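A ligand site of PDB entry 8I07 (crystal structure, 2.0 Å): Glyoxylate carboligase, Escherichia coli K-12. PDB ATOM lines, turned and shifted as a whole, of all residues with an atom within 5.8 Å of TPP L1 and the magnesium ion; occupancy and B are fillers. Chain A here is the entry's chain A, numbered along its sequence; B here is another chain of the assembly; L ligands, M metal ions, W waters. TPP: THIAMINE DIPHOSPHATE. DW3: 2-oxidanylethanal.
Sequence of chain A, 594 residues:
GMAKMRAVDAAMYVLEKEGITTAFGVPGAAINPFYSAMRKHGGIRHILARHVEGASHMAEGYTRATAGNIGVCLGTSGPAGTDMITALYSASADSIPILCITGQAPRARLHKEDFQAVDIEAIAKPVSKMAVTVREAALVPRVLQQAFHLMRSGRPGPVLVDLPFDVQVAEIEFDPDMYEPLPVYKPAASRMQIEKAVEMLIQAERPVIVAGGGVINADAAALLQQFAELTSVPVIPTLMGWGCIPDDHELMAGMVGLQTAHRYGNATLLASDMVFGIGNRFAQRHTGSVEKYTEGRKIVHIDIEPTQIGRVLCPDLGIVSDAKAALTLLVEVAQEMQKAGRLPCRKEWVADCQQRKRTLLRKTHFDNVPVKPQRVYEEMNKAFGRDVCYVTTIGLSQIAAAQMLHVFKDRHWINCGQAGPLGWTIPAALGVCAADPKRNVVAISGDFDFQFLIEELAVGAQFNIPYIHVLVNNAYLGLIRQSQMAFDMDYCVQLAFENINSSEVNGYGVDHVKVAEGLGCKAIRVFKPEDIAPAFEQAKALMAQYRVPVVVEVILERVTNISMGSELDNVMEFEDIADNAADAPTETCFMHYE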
ATOM      1  N   ILE A 394      -6.930 -24.127 -21.255  1.00  0.00           N
ATOM      2  CA  ILE A 394      -8.254 -24.716 -21.405  1.00  0.00           C
ATOM      3  C   ILE A 394      -9.285 -23.778 -20.789  1.00  0.00           C
ATOM      4  O   ILE A 394      -8.981 -22.985 -19.889  1.00  0.00           O
ATOM      5  CB  ILE A 394      -8.307 -26.126 -20.749  1.00  0.00           C
ATOM      6  CG1 ILE A 394      -9.624 -26.852 -21.075  1.00  0.00           C
ATOM      7  CG2 ILE A 394      -8.142 -26.033 -19.243  1.00  0.00           C
ATOM      8  CD1 ILE A 394      -9.587 -28.342 -20.794  1.00  0.00           C
ATOM      9  N   GLY A 395     -10.520 -23.887 -21.252  1.00  0.00           N
ATOM     10  CA  GLY A 395     -11.607 -23.015 -20.847  1.00  0.00           C
ATOM     11  C   GLY A 395     -12.280 -22.387 -22.062  1.00  0.00           C
ATOM     12  O   GLY A 395     -11.839 -22.540 -23.197  1.00  0.00           O
ATOM     13  N   LEU A 396     -13.394 -21.691 -21.796  1.00  0.00           N
ATOM     14  CA  LEU A 396     -14.002 -20.924 -22.885  1.00  0.00           C
ATOM     15  C   LEU A 396     -13.023 -19.879 -23.404  1.00  0.00           C
ATOM     16  O   LEU A 396     -12.991 -19.579 -24.609  1.00  0.00           O
ATOM     17  CB  LEU A 396     -15.315 -20.283 -22.425  1.00  0.00           C
ATOM     18  CG  LEU A 396     -16.443 -21.254 -22.068  1.00  0.00           C
ATOM     19  CD1 LEU A 396     -17.750 -20.486 -21.762  1.00  0.00           C
ATOM     20  CD2 LEU A 396     -16.662 -22.270 -23.174  1.00  0.00           C
ATOM     21  N   SER A 397     -12.195 -19.354 -22.515  1.00  0.00           N
ATOM     22  CA  SER A 397     -11.106 -18.470 -22.892  1.00  0.00           C
ATOM     23  C   SER A 397     -10.287 -19.078 -24.014  1.00  0.00           C
ATOM     24  O   SER A 397     -10.091 -18.452 -25.064  1.00  0.00           O
ATOM     25  CB  SER A 397     -10.223 -18.238 -21.665  1.00  0.00           C
ATOM     26  OG  SER A 397      -9.880 -19.528 -21.106  1.00  0.00           O
ATOM     27  N   GLN A 398      -9.810 -20.315 -23.816  1.00  0.00           N
ATOM     28  CA  GLN A 398      -8.927 -20.978 -24.771  1.00  0.00           C
ATOM     29  C   GLN A 398      -9.680 -21.475 -26.001  1.00  0.00           C
ATOM     30  O   GLN A 398      -9.145 -21.433 -27.116  1.00  0.00           O
ATOM     31  CB  GLN A 398      -8.184 -22.144 -24.102  1.00  0.00           C
ATOM     32  CG  GLN A 398      -7.398 -23.064 -25.059  1.00  0.00           C
ATOM     33  CD  GLN A 398      -8.131 -24.373 -25.397  1.00  0.00           C
ATOM     34  OE1 GLN A 398      -9.237 -24.609 -24.939  1.00  0.00           O
ATOM     35  NE2 GLN A 398      -7.496 -25.240 -26.213  1.00  0.00           N
ATOM     36  N   ALA A 419      -3.983 -32.875 -22.250  1.00  0.00           N
ATOM     37  CA  ALA A 419      -4.195 -32.939 -20.805  1.00  0.00           C
ATOM     38  C   ALA A 419      -4.861 -31.700 -20.216  1.00  0.00           C
ATOM     39  O   ALA A 419      -5.612 -31.819 -19.236  1.00  0.00           O
ATOM     40  CB  ALA A 419      -2.855 -33.189 -20.092  1.00  0.00           C
ATOM     41  N   GLY A 420      -4.568 -30.508 -20.727  1.00  0.00           N
ATOM     42  CA  GLY A 420      -5.258 -29.314 -20.278  1.00  0.00           C
ATOM     43  C   GLY A 420      -5.278 -29.027 -18.769  1.00  0.00           C
ATOM     44  O   GLY A 420      -6.309 -28.631 -18.229  1.00  0.00           O
ATOM     45  N   PRO A 421      -4.160 -29.202 -18.060  1.00  0.00           N
ATOM     46  CA  PRO A 421      -4.154 -28.895 -16.610  1.00  0.00           C
ATOM     47  C   PRO A 421      -4.283 -27.404 -16.335  1.00  0.00           C
ATOM     48  O   PRO A 421      -3.488 -26.596 -16.820  1.00  0.00           O
ATOM     49  CB  PRO A 421      -2.797 -29.420 -16.150  1.00  0.00           C
ATOM     50  CG  PRO A 421      -1.938 -29.350 -17.375  1.00  0.00           C
ATOM     51  CD  PRO A 421      -2.850 -29.660 -18.541  1.00  0.00           C
ATOM     52  N   LEU A 422      -5.259 -27.043 -15.495  1.00  0.00           N
ATOM     53  CA  LEU A 422      -5.395 -25.651 -15.108  1.00  0.00           C
ATOM     54  C   LEU A 422      -4.161 -25.193 -14.348  1.00  0.00           C
ATOM     55  O   LEU A 422      -3.520 -25.959 -13.643  1.00  0.00           O
ATOM     56  CB  LEU A 422      -6.663 -25.442 -14.259  1.00  0.00           C
ATOM     57  CG  LEU A 422      -7.982 -25.496 -15.034  1.00  0.00           C
ATOM     58  CD1 LEU A 422      -9.137 -25.762 -14.068  1.00  0.00           C
ATOM     59  CD2 LEU A 422      -8.240 -24.207 -15.885  1.00  0.00           C
ATOM     60  N   SER A 445      -5.692 -16.567 -20.568  1.00  0.00           N
ATOM     61  CA  SER A 445      -6.272 -17.361 -19.481  1.00  0.00           C
ATOM     62  C   SER A 445      -7.659 -16.841 -19.168  1.00  0.00           C
ATOM     63  O   SER A 445      -7.921 -15.639 -19.263  1.00  0.00           O
ATOM     64  CB  SER A 445      -5.473 -17.262 -18.163  1.00  0.00           C
ATOM     65  OG  SER A 445      -4.266 -17.995 -18.172  1.00  0.00           O
ATOM     66  N   GLY A 446      -8.540 -17.756 -18.711  1.00  0.00           N
ATOM     67  CA  GLY A 446      -9.669 -17.360 -17.892  1.00  0.00           C
ATOM     68  C   GLY A 446      -9.258 -17.150 -16.435  1.00  0.00           C
ATOM     69  O   GLY A 446      -8.126 -17.452 -16.047  1.00  0.00           O
ATOM     70  N   ASP A 447     -10.193 -16.629 -15.622  1.00  0.00           N
ATOM     71  CA  ASP A 447      -9.842 -16.297 -14.244  1.00  0.00           C
ATOM     72  C   ASP A 447      -9.435 -17.533 -13.439  1.00  0.00           C
ATOM     73  O   ASP A 447      -8.493 -17.471 -12.631  1.00  0.00           O
ATOM     74  CB  ASP A 447     -10.964 -15.523 -13.530  1.00  0.00           C
ATOM     75  CG  ASP A 447     -12.372 -16.064 -13.809  1.00  0.00           C
ATOM     76  OD1 ASP A 447     -12.725 -16.404 -14.959  1.00  0.00           O
ATOM     77  OD2 ASP A 447     -13.168 -16.077 -12.851  1.00  0.00           O
ATOM     78  N   PHE A 448     -10.107 -18.662 -13.646  1.00  0.00           N
ATOM     79  CA  PHE A 448      -9.838 -19.840 -12.804  1.00  0.00           C
ATOM     80  C   PHE A 448      -8.458 -20.412 -13.109  1.00  0.00           C
ATOM     81  O   PHE A 448      -7.662 -20.657 -12.204  1.00  0.00           O
ATOM     82  CB  PHE A 448     -10.934 -20.880 -13.027  1.00  0.00           C
ATOM     83  CG  PHE A 448     -11.062 -21.926 -11.914  1.00  0.00           C
ATOM     84  CD1 PHE A 448     -11.156 -21.538 -10.590  1.00  0.00           C
ATOM     85  CD2 PHE A 448     -11.163 -23.258 -12.227  1.00  0.00           C
ATOM     86  CE1 PHE A 448     -11.311 -22.494  -9.565  1.00  0.00           C
ATOM     87  CE2 PHE A 448     -11.323 -24.225 -11.227  1.00  0.00           C
ATOM     88  CZ  PHE A 448     -11.408 -23.832  -9.884  1.00  0.00           C
ATOM     89  N   ASP A 449      -8.130 -20.567 -14.404  1.00  0.00           N
ATOM     90  CA  ASP A 449      -6.800 -20.993 -14.801  1.00  0.00           C
ATOM     91  C   ASP A 449      -5.732 -20.051 -14.263  1.00  0.00           C
ATOM     92  O   ASP A 449      -4.695 -20.492 -13.756  1.00  0.00           O
ATOM     93  CB  ASP A 449      -6.748 -21.070 -16.341  1.00  0.00           C
ATOM     94  CG  ASP A 449      -5.337 -21.112 -16.910  1.00  0.00           C
ATOM     95  OD1 ASP A 449      -4.467 -21.864 -16.433  1.00  0.00           O
ATOM     96  OD2 ASP A 449      -5.107 -20.423 -17.921  1.00  0.00           O
ATOM     97  N   PHE A 450      -5.987 -18.743 -14.332  1.00  0.00           N
ATOM     98  CA  PHE A 450      -5.032 -17.745 -13.861  1.00  0.00           C
ATOM     99  C   PHE A 450      -4.764 -17.891 -12.357  1.00  0.00           C
ATOM    100  O   PHE A 450      -3.639 -17.664 -11.901  1.00  0.00           O
ATOM    101  CB  PHE A 450      -5.573 -16.345 -14.179  1.00  0.00           C
ATOM    102  CG  PHE A 450      -4.565 -15.231 -14.035  1.00  0.00           C
ATOM    103  CD1 PHE A 450      -3.537 -15.092 -14.936  1.00  0.00           C
ATOM    104  CD2 PHE A 450      -4.706 -14.300 -13.022  1.00  0.00           C
ATOM    105  CE1 PHE A 450      -2.628 -14.059 -14.805  1.00  0.00           C
ATOM    106  CE2 PHE A 450      -3.800 -13.259 -12.901  1.00  0.00           C
ATOM    107  CZ  PHE A 450      -2.764 -13.138 -13.781  1.00  0.00           C
ATOM    108  N   PHE A 452      -4.917 -20.745 -10.389  1.00  0.00           N
ATOM    109  CA  PHE A 452      -4.305 -21.990  -9.906  1.00  0.00           C
ATOM    110  C   PHE A 452      -2.848 -21.784  -9.479  1.00  0.00           C
ATOM    111  O   PHE A 452      -2.451 -22.168  -8.369  1.00  0.00           O
ATOM    112  CB  PHE A 452      -4.360 -23.069 -10.989  1.00  0.00           C
ATOM    113  CG  PHE A 452      -5.480 -24.072 -10.837  1.00  0.00           C
ATOM    114  CD1 PHE A 452      -6.810 -23.653 -10.847  1.00  0.00           C
ATOM    115  CD2 PHE A 452      -5.214 -25.425 -10.750  1.00  0.00           C
ATOM    116  CE1 PHE A 452      -7.842 -24.581 -10.732  1.00  0.00           C
ATOM    117  CE2 PHE A 452      -6.230 -26.350 -10.638  1.00  0.00           C
ATOM    118  CZ  PHE A 452      -7.550 -25.926 -10.629  1.00  0.00           C
ATOM    119  N   VAL A 472      -9.212 -13.031 -19.260  1.00  0.00           N
ATOM    120  CA  VAL A 472     -10.617 -12.746 -19.567  1.00  0.00           C
ATOM    121  C   VAL A 472     -11.442 -13.284 -18.408  1.00  0.00           C
ATOM    122  O   VAL A 472     -11.530 -14.503 -18.205  1.00  0.00           O
ATOM    123  CB  VAL A 472     -11.045 -13.321 -20.924  1.00  0.00           C
ATOM    124  CG1 VAL A 472     -10.208 -12.700 -22.049  1.00  0.00           C
ATOM    125  CG2 VAL A 472     -10.945 -14.864 -20.987  1.00  0.00           C
ATOM    126  N   ASN A 473     -12.047 -12.370 -17.640  1.00  0.00           N
ATOM    127  CA  ASN A 473     -12.578 -12.670 -16.309  1.00  0.00           C
ATOM    128  C   ASN A 473     -14.101 -12.672 -16.354  1.00  0.00           C
ATOM    129  O   ASN A 473     -14.715 -11.622 -16.523  1.00  0.00           O
ATOM    130  CB  ASN A 473     -12.063 -11.640 -15.294  1.00  0.00           C
ATOM    131  CG  ASN A 473     -12.567 -11.892 -13.887  1.00  0.00           C
ATOM    132  OD1 ASN A 473     -13.212 -12.899 -13.622  1.00  0.00           O
ATOM    133  ND2 ASN A 473     -12.259 -10.986 -12.974  1.00  0.00           N
ATOM    134  N   ASN A 474     -14.705 -13.854 -16.185  1.00  0.00           N
ATOM    135  CA  ASN A 474     -16.150 -13.950 -16.080  1.00  0.00           C
ATOM    136  C   ASN A 474     -16.617 -14.382 -14.689  1.00  0.00           C
ATOM    137  O   ASN A 474     -17.788 -14.710 -14.507  1.00  0.00           O
ATOM    138  CB  ASN A 474     -16.698 -14.901 -17.161  1.00  0.00           C
ATOM    139  CG  ASN A 474     -16.047 -16.297 -17.148  1.00  0.00           C
ATOM    140  OD1 ASN A 474     -15.434 -16.707 -16.162  1.00  0.00           O
ATOM    141  ND2 ASN A 474     -16.176 -17.020 -18.259  1.00  0.00           N
ATOM    142  N   ALA A 475     -15.730 -14.400 -13.700  1.00  0.00           N
ATOM    143  CA  ALA A 475     -16.046 -14.913 -12.361  1.00  0.00           C
ATOM    144  C   ALA A 475     -16.770 -16.257 -12.439  1.00  0.00           C
ATOM    145  O   ALA A 475     -17.674 -16.543 -11.651  1.00  0.00           O
ATOM    146  CB  ALA A 475     -16.845 -13.892 -11.552  1.00  0.00           C
ATOM    147  N   TYR A 476     -16.334 -17.109 -13.361  1.00  0.00           N
ATOM    148  CA  TYR A 476     -16.989 -18.396 -13.605  1.00  0.00           C
ATOM    149  C   TYR A 476     -15.936 -19.414 -14.021  1.00  0.00           C
ATOM    150  O   TYR A 476     -14.931 -19.065 -14.635  1.00  0.00           O
ATOM    151  CB  TYR A 476     -18.031 -18.280 -14.734  1.00  0.00           C
ATOM    152  CG  TYR A 476     -19.519 -18.304 -14.396  1.00  0.00           C
ATOM    153  CD1 TYR A 476     -20.157 -19.481 -14.054  1.00  0.00           C
ATOM    154  CD2 TYR A 476     -20.291 -17.152 -14.505  1.00  0.00           C
ATOM    155  CE1 TYR A 476     -21.518 -19.500 -13.785  1.00  0.00           C
ATOM    156  CE2 TYR A 476     -21.641 -17.166 -14.263  1.00  0.00           C
ATOM    157  CZ  TYR A 476     -22.254 -18.338 -13.888  1.00  0.00           C
ATOM    158  OH  TYR A 476     -23.614 -18.354 -13.636  1.00  0.00           O
ATOM    159  N   LEU A 477     -16.188 -20.699 -13.711  1.00  0.00           N
ATOM    160  CA  LEU A 477     -15.607 -21.776 -14.516  1.00  0.00           C
ATOM    161  C   LEU A 477     -16.530 -21.922 -15.726  1.00  0.00           C
ATOM    162  O   LEU A 477     -17.487 -22.705 -15.736  1.00  0.00           O
ATOM    163  CB  LEU A 477     -15.476 -23.096 -13.749  1.00  0.00           C
ATOM    164  CG  LEU A 477     -15.289 -23.233 -12.228  1.00  0.00           C
ATOM    165  CD1 LEU A 477     -14.843 -24.647 -11.803  1.00  0.00           C
ATOM    166  CD2 LEU A 477     -14.443 -22.139 -11.585  1.00  0.00           C
ATOM    167  N   GLY A 478     -16.298 -21.089 -16.735  1.00  0.00           N
ATOM    168  CA  GLY A 478     -17.304 -20.905 -17.767  1.00  0.00           C
ATOM    169  C   GLY A 478     -17.537 -22.146 -18.607  1.00  0.00           C
ATOM    170  O   GLY A 478     -18.679 -22.491 -18.926  1.00  0.00           O
ATOM    171  N   LEU A 479     -16.467 -22.875 -18.930  1.00  0.00           N
ATOM    172  CA  LEU A 479     -16.653 -24.092 -19.703  1.00  0.00           C
ATOM    173  C   LEU A 479     -17.492 -25.106 -18.917  1.00  0.00           C
ATOM    174  O   LEU A 479     -18.333 -25.798 -19.495  1.00  0.00           O
ATOM    175  CB  LEU A 479     -15.293 -24.696 -20.092  1.00  0.00           C
ATOM    176  CG  LEU A 479     -15.317 -26.004 -20.899  1.00  0.00           C
ATOM    177  CD1 LEU A 479     -16.137 -25.867 -22.173  1.00  0.00           C
ATOM    178  CD2 LEU A 479     -13.898 -26.468 -21.217  1.00  0.00           C
ATOM    179  N   ILE A 480     -17.310 -25.160 -17.600  1.00  0.00           N
ATOM    180  CA  ILE A 480     -18.055 -26.152 -16.830  1.00  0.00           C
ATOM    181  C   ILE A 480     -19.497 -25.714 -16.684  1.00  0.00           C
ATOM    182  O   ILE A 480     -20.409 -26.539 -16.762  1.00  0.00           O
ATOM    183  CB  ILE A 480     -17.380 -26.416 -15.458  1.00  0.00           C
ATOM    184  CG1 ILE A 480     -15.877 -26.666 -15.653  1.00  0.00           C
ATOM    185  CG2 ILE A 480     -18.026 -27.628 -14.775  1.00  0.00           C
ATOM    186  CD1 ILE A 480     -15.552 -27.675 -16.755  1.00  0.00           C
ATOM    187  N   LEU A 495     -17.354 -18.014  -9.094  1.00  0.00           N
ATOM    188  CA  LEU A 495     -16.223 -17.528  -8.322  1.00  0.00           C
ATOM    189  C   LEU A 495     -16.460 -16.142  -7.746  1.00  0.00           C
ATOM    190  O   LEU A 495     -15.571 -15.612  -7.062  1.00  0.00           O
ATOM    191  CB  LEU A 495     -14.966 -17.517  -9.198  1.00  0.00           C
ATOM    192  CG  LEU A 495     -14.481 -18.879  -9.691  1.00  0.00           C
ATOM    193  CD1 LEU A 495     -13.421 -18.730 -10.764  1.00  0.00           C
ATOM    194  CD2 LEU A 495     -13.956 -19.757  -8.512  1.00  0.00           C
ATOM    195  N   VAL B  26     -13.397 -29.426  -7.362  1.00  0.00           N
ATOM    196  CA  VAL B  26     -13.381 -28.621  -8.581  1.00  0.00           C
ATOM    197  C   VAL B  26     -14.146 -29.414  -9.639  1.00  0.00           C
ATOM    198  O   VAL B  26     -13.675 -30.489 -10.049  1.00  0.00           O
ATOM    199  CB  VAL B  26     -11.946 -28.323  -9.047  1.00  0.00           C
ATOM    200  CG1 VAL B  26     -11.960 -27.577 -10.415  1.00  0.00           C
ATOM    201  CG2 VAL B  26     -11.182 -27.530  -7.988  1.00  0.00           C
ATOM    202  N   PRO B  27     -15.330 -28.969 -10.055  1.00  0.00           N
ATOM    203  CA  PRO B  27     -16.096 -29.744 -11.051  1.00  0.00           C
ATOM    204  C   PRO B  27     -15.444 -29.680 -12.434  1.00  0.00           C
ATOM    205  O   PRO B  27     -14.560 -28.868 -12.703  1.00  0.00           O
ATOM    206  CB  PRO B  27     -17.471 -29.058 -11.049  1.00  0.00           C
ATOM    207  CG  PRO B  27     -17.165 -27.629 -10.693  1.00  0.00           C
ATOM    208  CD  PRO B  27     -16.008 -27.700  -9.709  1.00  0.00           C
ATOM    209  N   GLY B  28     -15.843 -30.631 -13.276  1.00  0.00           N
ATOM    210  CA  GLY B  28     -15.466 -30.647 -14.683  1.00  0.00           C
ATOM    211  C   GLY B  28     -16.447 -31.527 -15.408  1.00  0.00           C
ATOM    212  O   GLY B  28     -17.299 -32.175 -14.796  1.00  0.00           O
ATOM    213  N   ALA B  29     -16.302 -31.591 -16.736  1.00  0.00           N
ATOM    214  CA  ALA B  29     -17.305 -32.278 -17.553  1.00  0.00           C
ATOM    215  C   ALA B  29     -17.466 -33.740 -17.152  1.00  0.00           C
ATOM    216  O   ALA B  29     -18.592 -34.253 -17.086  1.00  0.00           O
ATOM    217  CB  ALA B  29     -16.924 -32.152 -19.035  1.00  0.00           C
ATOM    218  N   VAL B  52      -6.948 -27.869  -7.619  1.00  0.00           N
ATOM    219  CA  VAL B  52      -7.344 -29.212  -7.192  1.00  0.00           C
ATOM    220  C   VAL B  52      -6.461 -29.667  -6.044  1.00  0.00           C
ATOM    221  O   VAL B  52      -6.930 -30.340  -5.125  1.00  0.00           O
ATOM    222  CB  VAL B  52      -7.306 -30.208  -8.363  1.00  0.00           C
ATOM    223  CG1 VAL B  52      -7.359 -31.645  -7.858  1.00  0.00           C
ATOM    224  CG2 VAL B  52      -8.485 -29.957  -9.318  1.00  0.00           C
ATOM    225  N   THR B  76     -12.401 -33.754 -11.664  1.00  0.00           N
ATOM    226  CA  THR B  76     -12.748 -34.283 -12.975  1.00  0.00           C
ATOM    227  C   THR B  76     -11.681 -35.304 -13.408  1.00  0.00           C
ATOM    228  O   THR B  76     -10.879 -35.787 -12.591  1.00  0.00           O
ATOM    229  CB  THR B  76     -12.939 -33.129 -13.966  1.00  0.00           C
ATOM    230  OG1 THR B  76     -13.683 -33.583 -15.099  1.00  0.00           O
ATOM    231  CG2 THR B  76     -11.594 -32.561 -14.430  1.00  0.00           C
ATOM    232  N   PRO B  79      -6.029 -34.331 -15.557  1.00  0.00           N
ATOM    233  CA  PRO B  79      -5.105 -33.641 -14.635  1.00  0.00           C
ATOM    234  C   PRO B  79      -5.658 -33.445 -13.221  1.00  0.00           C
ATOM    235  O   PRO B  79      -4.876 -33.161 -12.302  1.00  0.00           O
ATOM    236  CB  PRO B  79      -4.834 -32.299 -15.328  1.00  0.00           C
ATOM    237  CG  PRO B  79      -6.108 -32.041 -16.086  1.00  0.00           C
ATOM    238  CD  PRO B  79      -6.513 -33.425 -16.615  1.00  0.00           C
ATOM    239  N   ALA B  80      -6.970 -33.514 -13.008  1.00  0.00           N
ATOM    240  CA  ALA B  80      -7.490 -33.421 -11.649  1.00  0.00           C
ATOM    241  C   ALA B  80      -6.964 -34.558 -10.780  1.00  0.00           C
ATOM    242  O   ALA B  80      -6.457 -34.328  -9.687  1.00  0.00           O
ATOM    243  CB  ALA B  80      -9.030 -33.423 -11.661  1.00  0.00           C
ATOM    244  N   ASP B  83      -3.353 -34.076  -9.972  1.00  0.00           N
ATOM    245  CA  ASP B  83      -3.204 -33.034  -8.951  1.00  0.00           C
ATOM    246  C   ASP B  83      -3.556 -33.520  -7.540  1.00  0.00           C
ATOM    247  O   ASP B  83      -3.410 -32.731  -6.599  1.00  0.00           O
ATOM    248  CB  ASP B  83      -4.092 -31.825  -9.274  1.00  0.00           C
ATOM    249  CG  ASP B  83      -3.494 -30.900 -10.318  1.00  0.00           C
ATOM    250  OD1 ASP B  83      -2.324 -31.060 -10.738  1.00  0.00           O
ATOM    251  OD2 ASP B  83      -4.236 -29.998 -10.738  1.00  0.00           O
ATOM    252  N   GLN B 116      -8.253 -35.749 -21.998  1.00  0.00           N
ATOM    253  CA  GLN B 116      -8.119 -35.710 -20.535  1.00  0.00           C
ATOM    254  C   GLN B 116      -8.463 -37.042 -19.865  1.00  0.00           C
ATOM    255  O   GLN B 116      -9.165 -37.086 -18.861  1.00  0.00           O
ATOM    256  CB  GLN B 116      -8.989 -34.582 -19.945  1.00  0.00           C
ATOM    257  CG  GLN B 116      -8.474 -33.192 -20.263  1.00  0.00           C
ATOM    258  CD  GLN B 116      -9.106 -32.105 -19.385  1.00  0.00           C
ATOM    259  OE1 GLN B 116     -10.330 -32.063 -19.209  1.00  0.00           O
ATOM    260  NE2 GLN B 116      -8.273 -31.203 -18.854  1.00  0.00           N
HETATM  261  N1' TPP L   1      -9.172 -29.462 -12.889  1.00  0.00           N
HETATM  262  C2' TPP L   1      -8.001 -29.353 -13.545  1.00  0.00           C
HETATM  263  CM2 TPP L   1      -6.752 -29.506 -12.742  1.00  0.00           C
HETATM  264  N3' TPP L   1      -7.852 -29.109 -14.854  1.00  0.00           N
HETATM  265  C4' TPP L   1      -8.975 -28.981 -15.589  1.00  0.00           C
HETATM  266  N4' TPP L   1      -8.807 -28.748 -16.903  1.00  0.00           N
HETATM  267  C5' TPP L   1     -10.278 -29.040 -14.979  1.00  0.00           C
HETATM  268  C6' TPP L   1     -10.276 -29.309 -13.629  1.00  0.00           C
HETATM  269  C7' TPP L   1     -11.587 -28.914 -15.745  1.00  0.00           C
HETATM  270  N3  TPP L   1     -11.816 -27.581 -16.356  1.00  0.00           N
HETATM  271  C2  TPP L   1     -11.654 -27.324 -17.649  1.00  0.00           C
HETATM  272  S1  TPP L   1     -12.034 -25.725 -18.052  1.00  0.00           S
HETATM  273  C5  TPP L   1     -12.483 -25.386 -16.419  1.00  0.00           C
HETATM  274  C4  TPP L   1     -12.303 -26.488 -15.626  1.00  0.00           C
HETATM  275  CM4 TPP L   1     -12.559 -26.596 -14.164  1.00  0.00           C
HETATM  276  C6  TPP L   1     -12.932 -24.000 -16.042  1.00  0.00           C
HETATM  277  C7  TPP L   1     -12.091 -22.941 -16.708  1.00  0.00           C
HETATM  278  O7  TPP L   1     -12.356 -21.652 -16.087  1.00  0.00           O
HETATM  279  PA  TPP L   1     -11.610 -20.337 -16.488  1.00  0.00           P
HETATM  280  O1A TPP L   1     -10.102 -20.602 -16.539  1.00  0.00           O
HETATM  281  O2A TPP L   1     -12.160 -19.210 -15.701  1.00  0.00           O
HETATM  282  O3A TPP L   1     -12.167 -20.179 -17.967  1.00  0.00           O
HETATM  283  PB  TPP L   1     -13.556 -19.845 -18.652  1.00  0.00           P
HETATM  284  O1B TPP L   1     -14.466 -19.271 -17.609  1.00  0.00           O
HETATM  285  O2B TPP L   1     -13.222 -18.910 -19.775  1.00  0.00           O
HETATM  286  O3B TPP L   1     -14.074 -21.200 -19.130  1.00  0.00           O
HETATM  287  C02 DW3 L   2     -14.278 -29.792 -19.095  1.00  0.00           C
HETATM  288  C03 DW3 L   2     -14.542 -30.415 -20.474  1.00  0.00           C
HETATM  289  O01 DW3 L   2     -14.050 -30.480 -18.149  1.00  0.00           O
HETATM  290  O04 DW3 L   2     -13.420 -30.270 -21.299  1.00  0.00           O
HETATM  291 MG    MG M   1     -13.762 -17.884 -16.030  1.00  0.00          MG
HETATM  292  O   HOH W   1     -14.311 -16.767 -21.475  1.00  0.00           O
HETATM  293  O   HOH W   2     -12.888 -16.817 -17.834  1.00  0.00           O
HETATM  294  O   HOH W   3     -11.364 -31.070 -11.256  1.00  0.00           O
HETATM  295  O   HOH W   4      -8.943 -20.441 -18.824  1.00  0.00           O
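O of Ala 419 lies within hydrogen-bond range of NE2 of Gln 116 of chain B, 2.8 Å away. OG of Ser 445 is in hydrogen-bond range of OD2 of Asp 449, at 2.6 Å. The side-chain carboxylate (OD2) of Asp 447 sits close to the side-chain amide oxygen (OD1) of Asn 473 (3.3 Å). The side-chain carboxylate of Asp 447 lies close to the backbone NH of Ala 475. O of Gly 420 sits at hydrogen-bond distance from NE2 of Gln 116 of chain B (3.3 Å). The side-chain hydroxyl (OG) of Ser 397 sits at hydrogen-bond distance from the backbone NH (N) of Gly 446 (3.3 Å).
The magnesium ion is bound by OD1 of Asn 474 (2.0 Å). The side-chain carboxylate (OD1) of Asp 447 binds the magnesium ion (2.1 Å). O2A of TPP L1 is bound to the magnesium ion, 2.1 Å away. O of Tyr 476 binds the magnesium ion, 2.2 Å away. The magnesium ion is bound by O1B of TPP L1 (2.2 Å). Water W2 binds the magnesium ion (2.3 Å).
Merely in contact with TPP L1: Ile 394 (3.6 Å), Gly 395 (3.5 Å), Gly 446 (3.5 Å), Phe 452 (3.8 Å), Leu 477 (3.5 Å), Ile 480 (3.6 Å), Val 26 of chain B (3.9 Å), Pro 27 of chain B (3.4 Å), Val 52 of chain B (3.7 Å), Thr 76 of chain B (3.6 Å), Pro 79 of chain B (3.6 Å) and Asp 83 of chain B (3.3 Å). Within 4 Å of TPP L1: Ile 394, Gly 395, Leu 396, Ser 397, Gly 420, Leu 422, Gly 446, Asp 447, Phe 448, Asp 449, Phe 452, Asn 474, Tyr 476, Leu 477, Gly 478, Leu 479, Ile 480, Val 26 of chain B, Pro 27 of chain B, Val 52 of chain B, Thr 76 of chain B, Pro 79 of chain B, Asp 83 of chain B and Gln 116 of chain B.
Water W2 lies within hydrogen-bond range of the backbone carbonyl oxygen (O) of Val 472 (2.7 Å), an oxygen (O2B) of TPP L1 (2.9 Å), the side-chain amide nitrogen (ND2) of Asn 474 (3.3 Å) and the backbone NH (N) of Asp 447 (3.5 Å). Water W4 lies within hydrogen-bond range of O1A of TPP L1 (2.6 Å), OG of Ser 397 (2.6 Å), N of Gly 446 (2.7 Å) and O of Ile 394 (2.8 Å). Water W1 lies within hydrogen-bond range of O2B of TPP L1 (2.9 Å) and N of Ser 397 (3.5 Å). Water W3 lies within hydrogen-bond range of the backbone carbonyl oxygen of Val 26 of chain B, the backbone NH of Thr 76 of chain B and a nitrogen (N1') of TPP L1.
N of Leu 479 sits at hydrogen-bond distance from O3B of TPP L1, 2.9 Å away. NE2 of Gln 116 of chain B lies close to N4' of TPP L1 (3.2 Å). O of Gly 420 sits at hydrogen-bond distance from N4' of TPP L1 (2.8 Å). An oxygen (O1A) of TPP L1 is in hydrogen-bond range of the backbone NH (N) of Asp 449 (2.9 Å). N of Asp 447 lies close to O2A of TPP L1, 3.2 Å away. N of Gly 478 is in hydrogen-bond range of O3B of TPP L1 (3.3 Å). O3B of TPP L1 sits at hydrogen-bond distance from N of Leu 396 (2.8 Å). The backbone NH of Ser 397 lies within hydrogen-bond range of an oxygen (O2B) of TPP L1 (3.0 Å). The backbone NH (N) of Ala 29 of chain B lies within hydrogen-bond range of an oxygen (O01) of DW3 L2. The backbone NH (N) of Leu 422 lies within hydrogen-bond range of a nitrogen (N3') of TPP L1 (3.4 Å). O1A of TPP L1 is in hydrogen-bond range of N of Phe 448 (3.5 Å).
Along chain A the residues within 4 Å of the magnesium ion span positions 447 to 476.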
